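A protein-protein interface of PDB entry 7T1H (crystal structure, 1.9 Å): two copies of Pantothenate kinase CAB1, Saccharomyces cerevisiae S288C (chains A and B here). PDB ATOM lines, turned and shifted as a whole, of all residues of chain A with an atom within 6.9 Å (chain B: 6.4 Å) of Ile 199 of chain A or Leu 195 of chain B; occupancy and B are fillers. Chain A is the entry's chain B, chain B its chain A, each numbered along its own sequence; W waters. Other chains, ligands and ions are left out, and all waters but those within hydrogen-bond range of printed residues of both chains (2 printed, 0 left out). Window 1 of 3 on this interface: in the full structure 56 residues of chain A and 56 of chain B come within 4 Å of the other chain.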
ATOM      1  N   TRP A 193     -15.208   4.178  -4.569  1.00  0.00           N
ATOM      2  CA  TRP A 193     -15.401   5.657  -4.593  1.00  0.00           C
ATOM      3  C   TRP A 193     -14.995   6.191  -5.978  1.00  0.00           C
ATOM      4  O   TRP A 193     -15.739   7.014  -6.571  1.00  0.00           O
ATOM      5  CB  TRP A 193     -14.637   6.351  -3.434  1.00  0.00           C
ATOM      6  CG  TRP A 193     -14.943   5.808  -2.062  1.00  0.00           C
ATOM      7  CD1 TRP A 193     -16.141   5.312  -1.641  1.00  0.00           C
ATOM      8  CD2 TRP A 193     -14.047   5.704  -0.923  1.00  0.00           C
ATOM      9  NE1 TRP A 193     -16.053   4.914  -0.332  1.00  0.00           N
ATOM     10  CE2 TRP A 193     -14.782   5.128   0.135  1.00  0.00           C
ATOM     11  CE3 TRP A 193     -12.700   6.031  -0.681  1.00  0.00           C
ATOM     12  CZ2 TRP A 193     -14.218   4.848   1.388  1.00  0.00           C
ATOM     13  CZ3 TRP A 193     -12.144   5.767   0.559  1.00  0.00           C
ATOM     14  CH2 TRP A 193     -12.895   5.175   1.582  1.00  0.00           C
ATOM     15  N   GLY A 194     -13.883   5.677  -6.491  1.00  0.00           N
ATOM     16  CA  GLY A 194     -13.313   6.070  -7.788  1.00  0.00           C
ATOM     17  C   GLY A 194     -14.240   5.709  -8.933  1.00  0.00           C
ATOM     18  O   GLY A 194     -14.517   6.583  -9.778  1.00  0.00           O
ATOM     19  N   LEU A 195     -14.757   4.483  -8.957  1.00  0.00           N
ATOM     20  CA  LEU A 195     -15.615   4.008 -10.080  1.00  0.00           C
ATOM     21  C   LEU A 195     -16.923   4.787 -10.053  1.00  0.00           C
ATOM     22  O   LEU A 195     -17.336   5.246 -11.117  1.00  0.00           O
ATOM     23  CB  LEU A 195     -15.871   2.510  -9.970  1.00  0.00           C
ATOM     24  CG  LEU A 195     -14.683   1.625 -10.302  1.00  0.00           C
ATOM     25  CD1 LEU A 195     -14.943   0.208  -9.829  1.00  0.00           C
ATOM     26  CD2 LEU A 195     -14.385   1.668 -11.783  1.00  0.00           C
ATOM     27  N   LEU A 196     -17.551   4.912  -8.881  1.00  0.00           N
ATOM     28  CA  LEU A 196     -18.910   5.498  -8.788  1.00  0.00           C
ATOM     29  C   LEU A 196     -18.849   7.006  -9.066  1.00  0.00           C
ATOM     30  O   LEU A 196     -19.787   7.515  -9.681  1.00  0.00           O
ATOM     31  CB  LEU A 196     -19.524   5.176  -7.429  1.00  0.00           C
ATOM     32  CG  LEU A 196     -19.894   3.699  -7.234  1.00  0.00           C
ATOM     33  CD1 LEU A 196     -20.561   3.513  -5.889  1.00  0.00           C
ATOM     34  CD2 LEU A 196     -20.774   3.205  -8.372  1.00  0.00           C
ATOM     35  N   SER A 197     -17.773   7.672  -8.645  1.00  0.00           N
ATOM     36  CA  SER A 197     -17.489   9.102  -8.915  1.00  0.00           C
ATOM     37  C   SER A 197     -17.393   9.315 -10.430  1.00  0.00           C
ATOM     38  O   SER A 197     -18.113  10.174 -10.967  1.00  0.00           O
ATOM     39  CB  SER A 197     -16.215   9.517  -8.195  1.00  0.00           C
ATOM     40  OG  SER A 197     -15.832  10.820  -8.563  1.00  0.00           O
ATOM     41  N   LEU A 198     -16.524   8.560 -11.105  1.00  0.00           N
ATOM     42  CA  LEU A 198     -16.315   8.709 -12.565  1.00  0.00           C
ATOM     43  C   LEU A 198     -17.611   8.390 -13.319  1.00  0.00           C
ATOM     44  O   LEU A 198     -17.923   9.102 -14.287  1.00  0.00           O
ATOM     45  CB  LEU A 198     -15.169   7.804 -13.019  1.00  0.00           C
ATOM     46  CG  LEU A 198     -14.644   8.081 -14.426  1.00  0.00           C
ATOM     47  CD1 LEU A 198     -14.160   9.517 -14.561  1.00  0.00           C
ATOM     48  CD2 LEU A 198     -13.520   7.135 -14.776  1.00  0.00           C
ATOM     49  N   ILE A 199     -18.311   7.320 -12.933  1.00  0.00           N
ATOM     50  CA  ILE A 199     -19.481   6.821 -13.690  1.00  0.00           C
ATOM     51  C   ILE A 199     -20.674   7.739 -13.428  1.00  0.00           C
ATOM     52  O   ILE A 199     -21.390   8.021 -14.388  1.00  0.00           O
ATOM     53  CB  ILE A 199     -19.795   5.347 -13.333  1.00  0.00           C
ATOM     54  CG1 ILE A 199     -18.692   4.402 -13.826  1.00  0.00           C
ATOM     55  CG2 ILE A 199     -21.154   4.958 -13.882  1.00  0.00           C
ATOM     56  CD1 ILE A 199     -18.878   2.963 -13.433  1.00  0.00           C
ATOM     57  N   THR A 200     -20.966   8.068 -12.169  1.00  0.00           N
ATOM     58  CA  THR A 200     -22.269   8.667 -11.775  1.00  0.00           C
ATOM     59  C   THR A 200     -22.150  10.176 -11.568  1.00  0.00           C
ATOM     60  O   THR A 200     -23.191  10.851 -11.586  1.00  0.00           O
ATOM     61  CB  THR A 200     -22.843   8.000 -10.519  1.00  0.00           C
ATOM     62  OG1 THR A 200     -22.075   8.373  -9.374  1.00  0.00           O
ATOM     63  CG2 THR A 200     -22.939   6.502 -10.686  1.00  0.00           C
ATOM     64  N   GLY A 201     -20.936  10.678 -11.376  1.00  0.00           N
ATOM     65  CA  GLY A 201     -20.673  12.085 -11.028  1.00  0.00           C
ATOM     66  C   GLY A 201     -20.977  12.381  -9.564  1.00  0.00           C
ATOM     67  O   GLY A 201     -20.901  13.525  -9.205  1.00  0.00           O
ATOM     68  N   ALA A 202     -21.305  11.391  -8.736  1.00  0.00           N
ATOM     69  CA  ALA A 202     -21.571  11.578  -7.290  1.00  0.00           C
ATOM     70  C   ALA A 202     -20.328  12.193  -6.645  1.00  0.00           C
ATOM     71  O   ALA A 202     -19.212  11.782  -7.019  1.00  0.00           O
ATOM     72  CB  ALA A 202     -21.951  10.268  -6.649  1.00  0.00           C
ATOM     73  N   SER A 245     -21.096  -9.341 -11.769  1.00  0.00           N
ATOM     74  CA  SER A 245     -21.243  -7.902 -11.447  1.00  0.00           C
ATOM     75  C   SER A 245     -21.011  -7.060 -12.716  1.00  0.00           C
ATOM     76  O   SER A 245     -19.949  -7.237 -13.385  1.00  0.00           O
ATOM     77  CB  SER A 245     -20.305  -7.473 -10.344  1.00  0.00           C
ATOM     78  OG  SER A 245     -20.635  -8.102  -9.116  1.00  0.00           O
ATOM     79  N   PHE A 246     -21.965  -6.165 -13.031  1.00  0.00           N
ATOM     80  CA  PHE A 246     -21.943  -5.293 -14.228  1.00  0.00           C
ATOM     81  C   PHE A 246     -21.924  -6.112 -15.523  1.00  0.00           C
ATOM     82  O   PHE A 246     -21.647  -5.538 -16.572  1.00  0.00           O
ATOM     83  CB  PHE A 246     -20.736  -4.357 -14.161  1.00  0.00           C
ATOM     84  CG  PHE A 246     -21.062  -2.894 -14.202  1.00  0.00           C
ATOM     85  CD1 PHE A 246     -21.768  -2.301 -13.165  1.00  0.00           C
ATOM     86  CD2 PHE A 246     -20.596  -2.095 -15.230  1.00  0.00           C
ATOM     87  CE1 PHE A 246     -22.032  -0.947 -13.177  1.00  0.00           C
ATOM     88  CE2 PHE A 246     -20.866  -0.732 -15.243  1.00  0.00           C
ATOM     89  CZ  PHE A 246     -21.606  -0.167 -14.233  1.00  0.00           C
ATOM     90  N   VAL A 249     -24.030  -4.885 -18.706  1.00  0.00           N
ATOM     91  CA  VAL A 249     -23.716  -3.559 -19.290  1.00  0.00           C
ATOM     92  C   VAL A 249     -23.138  -3.740 -20.703  1.00  0.00           C
ATOM     93  O   VAL A 249     -23.681  -3.091 -21.614  1.00  0.00           O
ATOM     94  CB  VAL A 249     -22.847  -2.750 -18.316  1.00  0.00           C
ATOM     95  CG1 VAL A 249     -22.376  -1.431 -18.901  1.00  0.00           C
ATOM     96  CG2 VAL A 249     -23.619  -2.493 -17.028  1.00  0.00           C
ATOM     97  N   PHE A 250     -22.135  -4.600 -20.925  1.00  0.00           N
ATOM     98  CA  PHE A 250     -21.415  -4.690 -22.235  1.00  0.00           C
ATOM     99  C   PHE A 250     -22.416  -5.095 -23.333  1.00  0.00           C
ATOM    100  O   PHE A 250     -22.398  -4.473 -24.397  1.00  0.00           O
ATOM    101  CB  PHE A 250     -20.191  -5.621 -22.157  1.00  0.00           C
ATOM    102  CG  PHE A 250     -19.238  -5.578 -23.334  1.00  0.00           C
ATOM    103  CD1 PHE A 250     -18.904  -4.385 -23.951  1.00  0.00           C
ATOM    104  CD2 PHE A 250     -18.681  -6.743 -23.838  1.00  0.00           C
ATOM    105  CE1 PHE A 250     -18.034  -4.350 -25.034  1.00  0.00           C
ATOM    106  CE2 PHE A 250     -17.822  -6.712 -24.927  1.00  0.00           C
ATOM    107  CZ  PHE A 250     -17.491  -5.514 -25.517  1.00  0.00           C
ATOM    108  N   PHE A 282     -27.935   3.786 -18.067  1.00  0.00           N
ATOM    109  CA  PHE A 282     -27.993   2.945 -16.854  1.00  0.00           C
ATOM    110  C   PHE A 282     -28.301   3.839 -15.657  1.00  0.00           C
ATOM    111  O   PHE A 282     -27.752   4.951 -15.564  1.00  0.00           O
ATOM    112  CB  PHE A 282     -26.657   2.212 -16.711  1.00  0.00           C
ATOM    113  CG  PHE A 282     -26.321   1.346 -17.903  1.00  0.00           C
ATOM    114  CD1 PHE A 282     -26.970   0.142 -18.084  1.00  0.00           C
ATOM    115  CD2 PHE A 282     -25.467   1.788 -18.896  1.00  0.00           C
ATOM    116  CE1 PHE A 282     -26.719  -0.646 -19.195  1.00  0.00           C
ATOM    117  CE2 PHE A 282     -25.186   0.980 -19.989  1.00  0.00           C
ATOM    118  CZ  PHE A 282     -25.803  -0.246 -20.126  1.00  0.00           C
ATOM    119  N   ASN A 284     -28.152   5.412 -12.046  1.00  0.00           N
ATOM    120  CA  ASN A 284     -27.126   5.738 -11.030  1.00  0.00           C
ATOM    121  C   ASN A 284     -27.352   4.894  -9.780  1.00  0.00           C
ATOM    122  O   ASN A 284     -26.395   4.279  -9.308  1.00  0.00           O
ATOM    123  CB  ASN A 284     -27.047   7.249 -10.837  1.00  0.00           C
ATOM    124  CG  ASN A 284     -26.409   7.908 -12.043  1.00  0.00           C
ATOM    125  OD1 ASN A 284     -25.625   7.290 -12.749  1.00  0.00           O
ATOM    126  ND2 ASN A 284     -26.769   9.145 -12.316  1.00  0.00           N
ATOM    127  N   ILE A 287     -26.292   1.284 -10.487  1.00  0.00           N
ATOM    128  CA  ILE A 287     -24.817   1.191 -10.631  1.00  0.00           C
ATOM    129  C   ILE A 287     -24.179   1.211  -9.232  1.00  0.00           C
ATOM    130  O   ILE A 287     -23.222   0.416  -8.984  1.00  0.00           O
ATOM    131  CB  ILE A 287     -24.315   2.361 -11.505  1.00  0.00           C
ATOM    132  CG1 ILE A 287     -24.875   2.271 -12.929  1.00  0.00           C
ATOM    133  CG2 ILE A 287     -22.797   2.427 -11.477  1.00  0.00           C
ATOM    134  CD1 ILE A 287     -24.702   3.518 -13.735  1.00  0.00           C
ATOM    135  N   LEU A 291     -21.974  -1.989  -7.658  1.00  0.00           N
ATOM    136  CA  LEU A 291     -20.536  -1.886  -7.361  1.00  0.00           C
ATOM    137  C   LEU A 291     -20.335  -1.940  -5.847  1.00  0.00           C
ATOM    138  O   LEU A 291     -19.297  -2.480  -5.422  1.00  0.00           O
ATOM    139  CB  LEU A 291     -19.930  -0.642  -8.027  1.00  0.00           C
ATOM    140  CG  LEU A 291     -19.925  -0.669  -9.548  1.00  0.00           C
ATOM    141  CD1 LEU A 291     -19.075   0.463 -10.121  1.00  0.00           C
ATOM    142  CD2 LEU A 291     -19.446  -2.034 -10.071  1.00  0.00           C
ATOM    143  N   GLY B 190     -17.201 -10.304 -17.488  1.00  0.00           N
ATOM    144  CA  GLY B 190     -18.407  -9.463 -17.591  1.00  0.00           C
ATOM    145  C   GLY B 190     -18.227  -8.127 -16.898  1.00  0.00           C
ATOM    146  O   GLY B 190     -18.703  -7.099 -17.415  1.00  0.00           O
ATOM    147  N   THR B 191     -17.564  -8.140 -15.744  1.00  0.00           N
ATOM    148  CA  THR B 191     -17.272  -6.963 -14.910  1.00  0.00           C
ATOM    149  C   THR B 191     -16.274  -6.047 -15.645  1.00  0.00           C
ATOM    150  O   THR B 191     -16.559  -4.867 -15.807  1.00  0.00           O
ATOM    151  CB  THR B 191     -16.809  -7.453 -13.538  1.00  0.00           C
ATOM    152  OG1 THR B 191     -17.716  -8.471 -13.077  1.00  0.00           O
ATOM    153  CG2 THR B 191     -16.722  -6.331 -12.544  1.00  0.00           C
ATOM    154  N   LEU B 192     -15.148  -6.591 -16.067  1.00  0.00           N
ATOM    155  CA  LEU B 192     -14.127  -5.850 -16.841  1.00  0.00           C
ATOM    156  C   LEU B 192     -14.771  -5.233 -18.093  1.00  0.00           C
ATOM    157  O   LEU B 192     -14.594  -3.997 -18.295  1.00  0.00           O
ATOM    158  CB  LEU B 192     -13.019  -6.828 -17.199  1.00  0.00           C
ATOM    159  CG  LEU B 192     -11.881  -6.201 -17.997  1.00  0.00           C
ATOM    160  CD1 LEU B 192     -11.222  -5.120 -17.143  1.00  0.00           C
ATOM    161  CD2 LEU B 192     -10.914  -7.267 -18.461  1.00  0.00           C
ATOM    162  N   TRP B 193     -15.474  -6.048 -18.894  1.00  0.00           N
ATOM    163  CA  TRP B 193     -16.090  -5.627 -20.182  1.00  0.00           C
ATOM    164  C   TRP B 193     -17.156  -4.571 -19.921  1.00  0.00           C
ATOM    165  O   TRP B 193     -17.101  -3.531 -20.603  1.00  0.00           O
ATOM    166  CB  TRP B 193     -16.640  -6.793 -21.033  1.00  0.00           C
ATOM    167  CG  TRP B 193     -15.666  -7.919 -21.244  1.00  0.00           C
ATOM    168  CD1 TRP B 193     -14.323  -7.827 -21.494  1.00  0.00           C
ATOM    169  CD2 TRP B 193     -15.972  -9.330 -21.214  1.00  0.00           C
ATOM    170  NE1 TRP B 193     -13.762  -9.079 -21.596  1.00  0.00           N
ATOM    171  CE2 TRP B 193     -14.752 -10.023 -21.424  1.00  0.00           C
ATOM    172  CE3 TRP B 193     -17.156 -10.076 -21.045  1.00  0.00           C
ATOM    173  CZ2 TRP B 193     -14.694 -11.421 -21.452  1.00  0.00           C
ATOM    174  CZ3 TRP B 193     -17.088 -11.457 -21.059  1.00  0.00           C
ATOM    175  CH2 TRP B 193     -15.872 -12.115 -21.274  1.00  0.00           C
ATOM    176  N   GLY B 194     -18.036  -4.790 -18.942  1.00  0.00           N
ATOM    177  CA  GLY B 194     -19.114  -3.841 -18.605  1.00  0.00           C
ATOM    178  C   GLY B 194     -18.583  -2.488 -18.151  1.00  0.00           C
ATOM    179  O   GLY B 194     -19.070  -1.463 -18.640  1.00  0.00           O
ATOM    180  N   LEU B 195     -17.625  -2.470 -17.233  1.00  0.00           N
ATOM    181  CA  LEU B 195     -17.047  -1.219 -16.692  1.00  0.00           C
ATOM    182  C   LEU B 195     -16.305  -0.471 -17.818  1.00  0.00           C
ATOM    183  O   LEU B 195     -16.533   0.717 -17.950  1.00  0.00           O
ATOM    184  CB  LEU B 195     -16.095  -1.532 -15.542  1.00  0.00           C
ATOM    185  CG  LEU B 195     -16.749  -1.937 -14.225  1.00  0.00           C
ATOM    186  CD1 LEU B 195     -15.674  -2.368 -13.247  1.00  0.00           C
ATOM    187  CD2 LEU B 195     -17.576  -0.797 -13.651  1.00  0.00           C
ATOM    188  N   LEU B 196     -15.445  -1.134 -18.592  1.00  0.00           N
ATOM    189  CA  LEU B 196     -14.599  -0.418 -19.578  1.00  0.00           C
ATOM    190  C   LEU B 196     -15.447   0.043 -20.780  1.00  0.00           C
ATOM    191  O   LEU B 196     -15.139   1.132 -21.332  1.00  0.00           O
ATOM    192  CB  LEU B 196     -13.437  -1.304 -20.014  1.00  0.00           C
ATOM    193  CG  LEU B 196     -12.400  -1.516 -18.919  1.00  0.00           C
ATOM    194  CD1 LEU B 196     -11.276  -2.386 -19.433  1.00  0.00           C
ATOM    195  CD2 LEU B 196     -11.907  -0.184 -18.375  1.00  0.00           C
ATOM    196  N   SER B 197     -16.429  -0.749 -21.195  1.00  0.00           N
ATOM    197  CA  SER B 197     -17.336  -0.384 -22.314  1.00  0.00           C
ATOM    198  C   SER B 197     -18.049   0.906 -21.914  1.00  0.00           C
ATOM    199  O   SER B 197     -17.971   1.883 -22.691  1.00  0.00           O
ATOM    200  CB  SER B 197     -18.271  -1.505 -22.711  1.00  0.00           C
ATOM    201  OG  SER B 197     -19.247  -1.773 -21.726  1.00  0.00           O
ATOM    202  N   LEU B 198     -18.562   0.975 -20.684  1.00  0.00           N
ATOM    203  CA  LEU B 198     -19.374   2.127 -20.220  1.00  0.00           C
ATOM    204  C   LEU B 198     -18.466   3.344 -20.013  1.00  0.00           C
ATOM    205  O   LEU B 198     -18.859   4.449 -20.442  1.00  0.00           O
ATOM    206  CB  LEU B 198     -20.115   1.759 -18.942  1.00  0.00           C
ATOM    207  CG  LEU B 198     -20.869   2.913 -18.285  1.00  0.00           C
ATOM    208  CD1 LEU B 198     -21.887   3.514 -19.251  1.00  0.00           C
ATOM    209  CD2 LEU B 198     -21.547   2.459 -17.008  1.00  0.00           C
ATOM    210  N   ILE B 199     -17.316   3.153 -19.357  1.00  0.00           N
ATOM    211  CA  ILE B 199     -16.433   4.265 -18.934  1.00  0.00           C
ATOM    212  C   ILE B 199     -15.681   4.811 -20.158  1.00  0.00           C
ATOM    213  O   ILE B 199     -15.616   6.031 -20.273  1.00  0.00           O
ATOM    214  CB  ILE B 199     -15.467   3.845 -17.810  1.00  0.00           C
ATOM    215  CG1 ILE B 199     -16.214   3.613 -16.491  1.00  0.00           C
ATOM    216  CG2 ILE B 199     -14.363   4.898 -17.666  1.00  0.00           C
ATOM    217  CD1 ILE B 199     -15.421   2.870 -15.423  1.00  0.00           C
ATOM    218  N   THR B 200     -15.131   3.952 -21.011  1.00  0.00           N
ATOM    219  CA  THR B 200     -14.154   4.326 -22.069  1.00  0.00           C
ATOM    220  C   THR B 200     -14.782   4.366 -23.464  1.00  0.00           C
ATOM    221  O   THR B 200     -14.129   4.919 -24.359  1.00  0.00           O
ATOM    222  CB  THR B 200     -12.957   3.371 -22.141  1.00  0.00           C
ATOM    223  OG1 THR B 200     -13.389   2.142 -22.707  1.00  0.00           O
ATOM    224  CG2 THR B 200     -12.280   3.181 -20.806  1.00  0.00           C
ATOM    225  N   TYR B 268     -29.779   8.822 -14.684  1.00  0.00           N
ATOM    226  CA  TYR B 268     -29.087   7.963 -15.676  1.00  0.00           C
ATOM    227  C   TYR B 268     -27.662   8.435 -15.943  1.00  0.00           C
ATOM    228  O   TYR B 268     -27.379   9.628 -15.888  1.00  0.00           O
ATOM    229  CB  TYR B 268     -29.872   7.922 -16.979  1.00  0.00           C
ATOM    230  CG  TYR B 268     -31.102   7.061 -16.910  1.00  0.00           C
ATOM    231  CD1 TYR B 268     -31.029   5.680 -17.024  1.00  0.00           C
ATOM    232  CD2 TYR B 268     -32.350   7.636 -16.757  1.00  0.00           C
ATOM    233  CE1 TYR B 268     -32.171   4.892 -16.978  1.00  0.00           C
ATOM    234  CE2 TYR B 268     -33.499   6.860 -16.703  1.00  0.00           C
ATOM    235  CZ  TYR B 268     -33.414   5.486 -16.818  1.00  0.00           C
ATOM    236  OH  TYR B 268     -34.573   4.752 -16.766  1.00  0.00           O
ATOM    237  N   SER B 269     -26.781   7.477 -16.208  1.00  0.00           N
ATOM    238  CA  SER B 269     -25.414   7.724 -16.710  1.00  0.00           C
ATOM    239  C   SER B 269     -25.269   6.950 -18.017  1.00  0.00           C
ATOM    240  O   SER B 269     -25.950   5.920 -18.205  1.00  0.00           O
ATOM    241  CB  SER B 269     -24.359   7.326 -15.714  1.00  0.00           C
ATOM    242  OG  SER B 269     -24.312   8.238 -14.631  1.00  0.00           O
ATOM    243  N   SER B 270     -24.422   7.455 -18.892  1.00  0.00           N
ATOM    244  CA  SER B 270     -24.068   6.838 -20.186  1.00  0.00           C
ATOM    245  C   SER B 270     -22.595   7.121 -20.414  1.00  0.00           C
ATOM    246  O   SER B 270     -22.044   7.959 -19.677  1.00  0.00           O
ATOM    247  CB  SER B 270     -24.910   7.428 -21.288  1.00  0.00           C
ATOM    248  OG  SER B 270     -24.545   8.787 -21.478  1.00  0.00           O
ATOM    249  N   SER B 273     -22.318  10.791 -21.044  1.00  0.00           N
ATOM    250  CA  SER B 273     -22.365  11.626 -19.814  1.00  0.00           C
ATOM    251  C   SER B 273     -21.033  11.555 -19.056  1.00  0.00           C
ATOM    252  O   SER B 273     -20.609  12.584 -18.525  1.00  0.00           O
ATOM    253  CB  SER B 273     -23.572  11.279 -18.943  1.00  0.00           C
ATOM    254  OG  SER B 273     -23.395  10.065 -18.225  1.00  0.00           O
ATOM    255  N   ILE B 274     -20.379  10.397 -19.003  1.00  0.00           N
ATOM    256  CA  ILE B 274     -19.048  10.245 -18.349  1.00  0.00           C
ATOM    257  C   ILE B 274     -17.992  11.025 -19.141  1.00  0.00           C
ATOM    258  O   ILE B 274     -17.133  11.667 -18.495  1.00  0.00           O
ATOM    259  CB  ILE B 274     -18.685   8.760 -18.226  1.00  0.00           C
ATOM    260  CG1 ILE B 274     -19.708   8.027 -17.346  1.00  0.00           C
ATOM    261  CG2 ILE B 274     -17.265   8.607 -17.700  1.00  0.00           C
ATOM    262  CD1 ILE B 274     -19.787   6.535 -17.584  1.00  0.00           C
ATOM    263  N   ASN B 278     -16.323  14.537 -17.634  1.00  0.00           N
ATOM    264  CA  ASN B 278     -14.911  14.348 -17.208  1.00  0.00           C
ATOM    265  C   ASN B 278     -13.927  14.720 -18.315  1.00  0.00           C
ATOM    266  O   ASN B 278     -12.722  14.659 -18.033  1.00  0.00           O
ATOM    267  CB  ASN B 278     -14.660  12.917 -16.752  1.00  0.00           C
ATOM    268  CG  ASN B 278     -15.562  12.602 -15.580  1.00  0.00           C
ATOM    269  OD1 ASN B 278     -15.436  13.215 -14.516  1.00  0.00           O
ATOM    270  ND2 ASN B 278     -16.502  11.693 -15.779  1.00  0.00           N
ATOM    271  N   ILE B 287      -7.137   3.784 -17.770  1.00  0.00           N
ATOM    272  CA  ILE B 287      -8.360   3.171 -17.175  1.00  0.00           C
ATOM    273  C   ILE B 287      -8.437   1.687 -17.536  1.00  0.00           C
ATOM    274  O   ILE B 287      -8.692   0.863 -16.621  1.00  0.00           O
ATOM    275  CB  ILE B 287      -9.615   3.932 -17.618  1.00  0.00           C
ATOM    276  CG1 ILE B 287      -9.664   5.311 -16.970  1.00  0.00           C
ATOM    277  CG2 ILE B 287     -10.871   3.114 -17.317  1.00  0.00           C
ATOM    278  CD1 ILE B 287     -10.762   6.197 -17.538  1.00  0.00           C
ATOM    279  N   LEU B 291      -8.046  -1.453 -14.718  1.00  0.00           N
ATOM    280  CA  LEU B 291      -9.178  -2.390 -14.433  1.00  0.00           C
ATOM    281  C   LEU B 291      -8.834  -3.787 -14.939  1.00  0.00           C
ATOM    282  O   LEU B 291      -9.208  -4.776 -14.273  1.00  0.00           O
ATOM    283  CB  LEU B 291     -10.476  -1.839 -15.020  1.00  0.00           C
ATOM    284  CG  LEU B 291     -10.959  -0.577 -14.326  1.00  0.00           C
ATOM    285  CD1 LEU B 291     -12.400  -0.282 -14.693  1.00  0.00           C
ATOM    286  CD2 LEU B 291     -10.795  -0.667 -12.811  1.00  0.00           C
ATOM    287  N   ILE B 295      -9.031  -6.652 -12.006  1.00  0.00           N
ATOM    288  CA  ILE B 295      -9.856  -7.884 -12.177  1.00  0.00           C
ATOM    289  C   ILE B 295      -8.935  -9.108 -12.286  1.00  0.00           C
ATOM    290  O   ILE B 295      -9.232 -10.121 -11.628  1.00  0.00           O
ATOM    291  CB  ILE B 295     -10.808  -7.770 -13.374  1.00  0.00           C
ATOM    292  CG1 ILE B 295     -11.821  -6.629 -13.213  1.00  0.00           C
ATOM    293  CG2 ILE B 295     -11.506  -9.109 -13.637  1.00  0.00           C
ATOM    294  CD1 ILE B 295     -12.746  -6.778 -12.018  1.00  0.00           C
HETATM  295  O   HOH W   1     -22.482  10.247 -15.538  1.00  0.00           O
HETATM  296  O   HOH W   2     -20.461  -6.798 -19.329  1.00  0.00           O
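The side-chain hydroxyl (OG1) of Thr 191 of chain B sits at hydrogen-bond distance from the backbone carbonyl oxygen (O) of Ser 245 of chain A (2.6 Å). The backbone carbonyl oxygen (O) of Ile 199 of chain A sits at hydrogen-bond distance from the side-chain hydroxyl (OG) of Ser 269 of chain B. N of Ser 269 of chain B lies within hydrogen-bond range of O of Phe 282 of chain A. OG of Ser 269 of chain B lies within hydrogen-bond range of OD1 of Asn 284 of chain A, at 2.5 Å. The side-chain amide nitrogen (ND2) of Asn 278 of chain B lies within hydrogen-bond range of the backbone carbonyl oxygen (O) of Leu 198 of chain A, 3.3 Å away. The backbone carbonyl oxygen (O) of Phe 246 of chain A lies close to the backbone carbonyl oxygen (O) of Gly 190 of chain B, at 3.4 Å.
O of Trp 193 of chain B is in hydrogen-bond range of OG of Ser 197 of chain B (3.0 Å). The backbone carbonyl oxygen of Gly 194 of chain B lies within hydrogen-bond range of the side-chain hydroxyl of Ser 197 of chain B, 3.1 Å away. O of Ile 274 of chain B is in hydrogen-bond range of ND2 of Asn 278 of chain B (2.8 Å). The backbone carbonyl oxygen (O) of Leu 196 of chain A sits at hydrogen-bond distance from the side-chain hydroxyl (OG1) of Thr 200 of chain A, at 2.5 Å. N of Ala 202 of chain A lies within hydrogen-bond range of OG1 of Thr 200 of chain A, 3.2 Å away.
Leu 195 of chain A touches Ile 199 of chain B (CD2 to CD1, 3.97 Å). Ile 274 of chain B touches Leu 198 of chain A. O of Ile 199 of chain A touches CG1 of Ile 274 of chain B, 3.4 Å away. Leu 195 of chain B touches Phe 246 of chain A. Val 249 of chain A touches Gly 194 of chain B (CG1 to O, 3.3 Å). Val 249 of chain A touches Leu 198 of chain B. Phe 250 of chain A touches Trp 193 of chain B (CD2 to CB, 3.5 Å). Phe 250 of chain A touches Gly 194 of chain B. Tyr 268 of chain B touches Phe 282 of chain A. Asn 284 of chain A touches Tyr 268 of chain B.
Printed residues of chain B within 4 Å of Ile 199 of chain A: Leu 195, Ile 199, Ser 269 and Ile 274. Of the printed residues of chain A, Leu 195 of chain B touches Ile 199 (3.99 Å) and Phe 246 (3.6 Å). Of the printed residues of chain A, Ser 269 of chain B touches Ile 199, Thr 200, Phe 282 and Asn 284. Of the printed residues of chain A, Ile 274 of chain B touches Leu 198 (3.5 Å) and Ile 199 (3.4 Å). The nearest printed residue of chain B that does not touch Ile 199 of chain A is Leu 198 of chain B (4.02 Å).
Printed residues of chain A that touch a printed residue of chain B: Leu 195, Leu 198, Ile 199, Thr 200, Ser 245, Phe 246, Val 249, Phe 250, Phe 282 and Asn 284. Along chain A the printed residues that touch a printed residue of chain B span positions 195 to 284. Among the printed residues, 24 pairs touch across the chains. Among the printed residues, no Asp or Glu carboxylate lies within 4 Å of a Lys or Arg side-chain nitrogen of the other chain.
Leu 195 of chain A touches Ile 199 of chain B, and with the chains exchanged Ile 199 of chain A touches Leu 195 of chain B. Leu 198 of chain A touches Ile 199 of chain B, but with the chains exchanged Ile 199 of chain A does not touch Leu 198 of chain B (4.02 Å). Ile 199 of chain B touches its own counterpart, Ile 199 of chain A. 10 positions are printed for both chains. Of the 24 pairs that touch across the chains among the printed residues, 3 have their exchanged pair printed and touching as well.
Water W2 lies within hydrogen-bond range of the backbone carbonyl oxygen (O) of Gly 190 of chain B, the backbone NH (N) of Gly 194 of chain B, the backbone NH (N) of Phe 250 of chain A and the backbone carbonyl oxygen (O) of Phe 246 of chain A. Water W1 lies within hydrogen-bond range of the backbone carbonyl oxygen of Ile 199 of chain A, the side-chain hydroxyl of Ser 273 of chain B and the side-chain hydroxyl of Ser 269 of chain B.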
